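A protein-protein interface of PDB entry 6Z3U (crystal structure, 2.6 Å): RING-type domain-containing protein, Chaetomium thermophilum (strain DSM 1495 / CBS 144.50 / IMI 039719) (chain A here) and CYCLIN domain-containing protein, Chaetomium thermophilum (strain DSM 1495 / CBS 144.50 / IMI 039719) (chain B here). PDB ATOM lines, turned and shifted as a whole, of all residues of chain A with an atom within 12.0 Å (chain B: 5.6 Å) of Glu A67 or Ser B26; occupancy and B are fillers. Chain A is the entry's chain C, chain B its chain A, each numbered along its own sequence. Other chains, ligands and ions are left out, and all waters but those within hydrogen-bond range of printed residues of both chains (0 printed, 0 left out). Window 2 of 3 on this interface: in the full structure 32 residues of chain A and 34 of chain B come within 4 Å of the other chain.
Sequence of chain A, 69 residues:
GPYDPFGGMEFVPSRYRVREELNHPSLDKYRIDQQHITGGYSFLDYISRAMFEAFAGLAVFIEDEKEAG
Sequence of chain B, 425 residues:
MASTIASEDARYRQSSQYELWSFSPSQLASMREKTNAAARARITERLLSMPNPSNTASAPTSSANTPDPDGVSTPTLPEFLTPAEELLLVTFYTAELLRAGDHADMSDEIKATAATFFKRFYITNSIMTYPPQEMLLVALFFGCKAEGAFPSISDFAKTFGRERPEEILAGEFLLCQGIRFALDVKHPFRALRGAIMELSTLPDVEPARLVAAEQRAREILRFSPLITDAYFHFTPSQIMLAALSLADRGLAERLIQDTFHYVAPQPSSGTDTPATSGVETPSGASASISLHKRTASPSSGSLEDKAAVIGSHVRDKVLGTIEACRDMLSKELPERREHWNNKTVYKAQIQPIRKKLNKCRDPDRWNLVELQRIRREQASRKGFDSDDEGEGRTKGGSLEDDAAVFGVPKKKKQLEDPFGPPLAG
CG of Glu A63 touches CB of Ser B24 (3.9 Å). Glu A63 touches Pro B25. OE1 of Gln B27 touches O of Lys A66, at 3.6 Å. Ser B26 touches Glu A67.
The side-chain hydroxyl (OG) of Ser B24 lies within hydrogen-bond range of the side-chain amide oxygen (OE1) of Gln B27. The side-chain hydroxyl of Ser B30 lies within hydrogen-bond range of the backbone carbonyl oxygen of Ser B26 (3.3 Å).
The side-chain hydroxyl of Ser B24 sits at hydrogen-bond distance from the side-chain carboxylate of Glu A67, at 2.5 Å. The side-chain amide oxygen of Gln B27 lies close to the side-chain carboxylate of Glu A67, 3.3 Å away.
Val A60 touches none of the printed residues of chain B. Printed residues of chain B within 4 Å of Glu A63: Ser B24 and Pro B25. Of the printed residues of chain B, Lys A66 touches Gln B27 (3.6 Å). Of the printed residues of chain B, Glu A67 touches Ser B24, Ser B26 and Gln B27. Ala A68 touches none of the printed residues of chain B. Pro B25 touches just one residue of chain A: Glu A63. Of chain A, only Glu A67 comes within 4 Å of Ser B26. Of chain A, only Lys A66 (3.6 Å) and Glu A67 (3.3 Å) come within 4 Å of Gln B27. No residue of chain A comes within 4 Å of Leu B28. No residue of chain A comes within 4 Å of Ala B29. No residue of chain A comes within 4 Å of Ser B30. The nearest printed residue of chain B that does not touch Glu A67 is Pro B25 (5.9 Å).
Printed residues of chain A that touch a printed residue of chain B: Glu A63, Lys A66 and Glu A67. Hydrophobic or aromatic side chains of chain B that line the printed part of chain A: Pro B25.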
ATOM      1  N   VAL A  60      40.246   5.993  -0.941  1.00  0.00           N
ATOM      2  CA  VAL A  60      38.967   6.636  -0.659  1.00  0.00           C
ATOM      3  C   VAL A  60      38.369   7.020  -2.008  1.00  0.00           C
ATOM      4  O   VAL A  60      38.797   7.985  -2.641  1.00  0.00           O
ATOM      5  CB  VAL A  60      39.128   7.845   0.262  1.00  0.00           C
ATOM      6  CG1 VAL A  60      37.863   8.691   0.263  1.00  0.00           C
ATOM      7  CG2 VAL A  60      39.454   7.389   1.673  1.00  0.00           C
ATOM      8  N   PHE A  61      37.382   6.248  -2.455  1.00  0.00           N
ATOM      9  CA  PHE A  61      36.735   6.469  -3.747  1.00  0.00           C
ATOM     10  C   PHE A  61      35.499   7.325  -3.501  1.00  0.00           C
ATOM     11  O   PHE A  61      34.437   6.815  -3.135  1.00  0.00           O
ATOM     12  CB  PHE A  61      36.393   5.136  -4.399  1.00  0.00           C
ATOM     13  CG  PHE A  61      37.555   4.180  -4.456  1.00  0.00           C
ATOM     14  CD1 PHE A  61      38.738   4.543  -5.077  1.00  0.00           C
ATOM     15  CD2 PHE A  61      37.470   2.926  -3.871  1.00  0.00           C
ATOM     16  CE1 PHE A  61      39.810   3.671  -5.127  1.00  0.00           C
ATOM     17  CE2 PHE A  61      38.538   2.051  -3.916  1.00  0.00           C
ATOM     18  CZ  PHE A  61      39.710   2.424  -4.543  1.00  0.00           C
ATOM     19  N   ILE A  62      35.636   8.634  -3.717  1.00  0.00           N
ATOM     20  CA  ILE A  62      34.587   9.571  -3.321  1.00  0.00           C
ATOM     21  C   ILE A  62      33.304   9.297  -4.093  1.00  0.00           C
ATOM     22  O   ILE A  62      32.209   9.253  -3.517  1.00  0.00           O
ATOM     23  CB  ILE A  62      35.070  11.021  -3.516  1.00  0.00           C
ATOM     24  CG1 ILE A  62      36.090  11.377  -2.429  1.00  0.00           C
ATOM     25  CG2 ILE A  62      33.889  11.985  -3.515  1.00  0.00           C
ATOM     26  CD1 ILE A  62      36.737  12.740  -2.594  1.00  0.00           C
ATOM     27  N   GLU A  63      33.418   9.102  -5.408  1.00  0.00           N
ATOM     28  CA  GLU A  63      32.227   8.933  -6.236  1.00  0.00           C
ATOM     29  C   GLU A  63      31.439   7.696  -5.820  1.00  0.00           C
ATOM     30  O   GLU A  63      30.234   7.772  -5.556  1.00  0.00           O
ATOM     31  CB  GLU A  63      32.624   8.852  -7.710  1.00  0.00           C
ATOM     32  CG  GLU A  63      31.464   8.557  -8.649  1.00  0.00           C
ATOM     33  CD  GLU A  63      31.817   8.792 -10.107  1.00  0.00           C
ATOM     34  OE1 GLU A  63      30.956   8.541 -10.977  1.00  0.00           O
ATOM     35  OE2 GLU A  63      32.954   9.229 -10.382  1.00  0.00           O
ATOM     36  N   ASP A  64      32.109   6.544  -5.751  1.00  0.00           N
ATOM     37  CA  ASP A  64      31.410   5.304  -5.431  1.00  0.00           C
ATOM     38  C   ASP A  64      30.883   5.316  -4.001  1.00  0.00           C
ATOM     39  O   ASP A  64      29.765   4.857  -3.742  1.00  0.00           O
ATOM     40  CB  ASP A  64      32.343   4.114  -5.650  1.00  0.00           C
ATOM     41  CG  ASP A  64      32.797   3.991  -7.090  1.00  0.00           C
ATOM     42  OD1 ASP A  64      31.930   3.991  -7.990  1.00  0.00           O
ATOM     43  OD2 ASP A  64      34.020   3.897  -7.324  1.00  0.00           O
ATOM     44  N   GLU A  65      31.673   5.836  -3.059  1.00  0.00           N
ATOM     45  CA  GLU A  65      31.263   5.815  -1.658  1.00  0.00           C
ATOM     46  C   GLU A  65      30.046   6.700  -1.416  1.00  0.00           C
ATOM     47  O   GLU A  65      29.138   6.323  -0.667  1.00  0.00           O
ATOM     48  CB  GLU A  65      32.432   6.246  -0.771  1.00  0.00           C
ATOM     49  CG  GLU A  65      33.590   5.253  -0.744  1.00  0.00           C
ATOM     50  CD  GLU A  65      34.801   5.775   0.012  1.00  0.00           C
ATOM     51  OE1 GLU A  65      35.922   5.292  -0.253  1.00  0.00           O
ATOM     52  OE2 GLU A  65      34.632   6.668   0.870  1.00  0.00           O
ATOM     53  N   LYS A  66      30.006   7.880  -2.041  1.00  0.00           N
ATOM     54  CA  LYS A  66      28.917   8.817  -1.788  1.00  0.00           C
ATOM     55  C   LYS A  66      27.628   8.403  -2.488  1.00  0.00           C
ATOM     56  O   LYS A  66      26.536   8.646  -1.959  1.00  0.00           O
ATOM     57  CB  LYS A  66      29.324  10.227  -2.219  1.00  0.00           C
ATOM     58  CG  LYS A  66      30.358  10.880  -1.305  1.00  0.00           C
ATOM     59  CD  LYS A  66      29.784  11.170   0.080  1.00  0.00           C
ATOM     60  CE  LYS A  66      30.818  11.796   1.000  1.00  0.00           C
ATOM     61  NZ  LYS A  66      30.273  12.003   2.369  1.00  0.00           N
ATOM     62  N   GLU A  67      27.728   7.800  -3.674  1.00  0.00           N
ATOM     63  CA  GLU A  67      26.539   7.331  -4.377  1.00  0.00           C
ATOM     64  C   GLU A  67      25.938   6.092  -3.727  1.00  0.00           C
ATOM     65  O   GLU A  67      24.755   5.809  -3.938  1.00  0.00           O
ATOM     66  CB  GLU A  67      26.876   7.036  -5.841  1.00  0.00           C
ATOM     67  CG  GLU A  67      27.046   8.278  -6.707  1.00  0.00           C
ATOM     68  CD  GLU A  67      25.720   8.897  -7.123  1.00  0.00           C
ATOM     69  OE1 GLU A  67      24.729   8.148  -7.269  1.00  0.00           O
ATOM     70  OE2 GLU A  67      25.671  10.132  -7.308  1.00  0.00           O
ATOM     71  N   ALA A  68      26.724   5.351  -2.945  1.00  0.00           N
ATOM     72  CA  ALA A  68      26.231   4.158  -2.272  1.00  0.00           C
ATOM     73  C   ALA A  68      25.361   4.471  -1.063  1.00  0.00           C
ATOM     74  O   ALA A  68      24.695   3.564  -0.551  1.00  0.00           O
ATOM     75  CB  ALA A  68      27.406   3.281  -1.834  1.00  0.00           C
ATOM     76  N   GLY A  69      25.352   5.715  -0.593  1.00  0.00           N
ATOM     77  CA  GLY A  69      24.547   6.091   0.554  1.00  0.00           C
ATOM     78  C   GLY A  69      23.163   6.579   0.173  1.00  0.00           C
ATOM     79  O   GLY A  69      23.019   7.527  -0.600  1.00  0.00           O
ATOM     80  N   SER B  24      29.739  13.023  -5.819  1.00  0.00           N
ATOM     81  CA  SER B  24      29.883  12.455  -7.145  1.00  0.00           C
ATOM     82  C   SER B  24      29.552  13.509  -8.203  1.00  0.00           C
ATOM     83  O   SER B  24      28.802  14.451  -7.930  1.00  0.00           O
ATOM     84  CB  SER B  24      28.958  11.254  -7.311  1.00  0.00           C
ATOM     85  OG  SER B  24      27.599  11.658  -7.339  1.00  0.00           O
ATOM     86  N   PRO B  25      30.095  13.375  -9.409  1.00  0.00           N
ATOM     87  CA  PRO B  25      29.767  14.355 -10.458  1.00  0.00           C
ATOM     88  C   PRO B  25      28.274  14.523 -10.671  1.00  0.00           C
ATOM     89  O   PRO B  25      27.819  15.631 -10.980  1.00  0.00           O
ATOM     90  CB  PRO B  25      30.462  13.781 -11.700  1.00  0.00           C
ATOM     91  CG  PRO B  25      31.585  12.956 -11.156  1.00  0.00           C
ATOM     92  CD  PRO B  25      31.069  12.370  -9.874  1.00  0.00           C
ATOM     93  N   SER B  26      27.490  13.456 -10.501  1.00  0.00           N
ATOM     94  CA  SER B  26      26.044  13.582 -10.637  1.00  0.00           C
ATOM     95  C   SER B  26      25.464  14.411  -9.498  1.00  0.00           C
ATOM     96  O   SER B  26      24.578  15.244  -9.716  1.00  0.00           O
ATOM     97  CB  SER B  26      25.399  12.198 -10.679  1.00  0.00           C
ATOM     98  OG  SER B  26      24.009  12.287 -10.946  1.00  0.00           O
ATOM     99  N   GLN B  27      25.961  14.203  -8.278  1.00  0.00           N
ATOM    100  CA  GLN B  27      25.512  15.007  -7.147  1.00  0.00           C
ATOM    101  C   GLN B  27      25.905  16.468  -7.317  1.00  0.00           C
ATOM    102  O   GLN B  27      25.129  17.372  -6.985  1.00  0.00           O
ATOM    103  CB  GLN B  27      26.092  14.444  -5.850  1.00  0.00           C
ATOM    104  CG  GLN B  27      25.418  13.171  -5.367  1.00  0.00           C
ATOM    105  CD  GLN B  27      26.207  12.478  -4.272  1.00  0.00           C
ATOM    106  OE1 GLN B  27      26.593  11.318  -4.412  1.00  0.00           O
ATOM    107  NE2 GLN B  27      26.457  13.188  -3.178  1.00  0.00           N
ATOM    108  N   LEU B  28      27.111  16.719  -7.839  1.00  0.00           N
ATOM    109  CA  LEU B  28      27.570  18.094  -8.015  1.00  0.00           C
ATOM    110  C   LEU B  28      26.689  18.846  -9.003  1.00  0.00           C
ATOM    111  O   LEU B  28      26.308  19.995  -8.754  1.00  0.00           O
ATOM    112  CB  LEU B  28      29.024  18.102  -8.489  1.00  0.00           C
ATOM    113  CG  LEU B  28      29.864  19.320  -8.104  1.00  0.00           C
ATOM    114  CD1 LEU B  28      30.132  19.327  -6.611  1.00  0.00           C
ATOM    115  CD2 LEU B  28      31.172  19.343  -8.880  1.00  0.00           C
ATOM    116  N   ALA B  29      26.350  18.216 -10.127  1.00  0.00           N
ATOM    117  CA  ALA B  29      25.518  18.885 -11.118  1.00  0.00           C
ATOM    118  C   ALA B  29      24.143  19.205 -10.547  1.00  0.00           C
ATOM    119  O   ALA B  29      23.647  20.329 -10.684  1.00  0.00           O
ATOM    120  CB  ALA B  29      25.399  18.017 -12.371  1.00  0.00           C
ATOM    121  N   SER B  30      23.516  18.229  -9.885  1.00  0.00           N
ATOM    122  CA  SER B  30      22.176  18.443  -9.344  1.00  0.00           C
ATOM    123  C   SER B  30      22.151  19.606  -8.359  1.00  0.00           C
ATOM    124  O   SER B  30      21.227  20.429  -8.385  1.00  0.00           O
ATOM    125  CB  SER B  30      21.671  17.160  -8.682  1.00  0.00           C
ATOM    126  OG  SER B  30      21.451  16.149  -9.649  1.00  0.00           O
ATOM    127  N   MET B  31      23.154  19.694  -7.483  1.00  0.00           N
ATOM    128  CA  MET B  31      23.234  20.826  -6.563  1.00  0.00           C
ATOM    129  C   MET B  31      23.336  22.148  -7.313  1.00  0.00           C
ATOM    130  O   MET B  31      22.592  23.094  -7.029  1.00  0.00           O
ATOM    131  CB  MET B  31      24.424  20.652  -5.615  1.00  0.00           C
ATOM    132  CG  MET B  31      24.148  19.700  -4.469  1.00  0.00           C
ATOM    133  SD  MET B  31      25.451  19.674  -3.232  1.00  0.00           S
ATOM    134  CE  MET B  31      26.615  18.567  -4.008  1.00  0.00           C
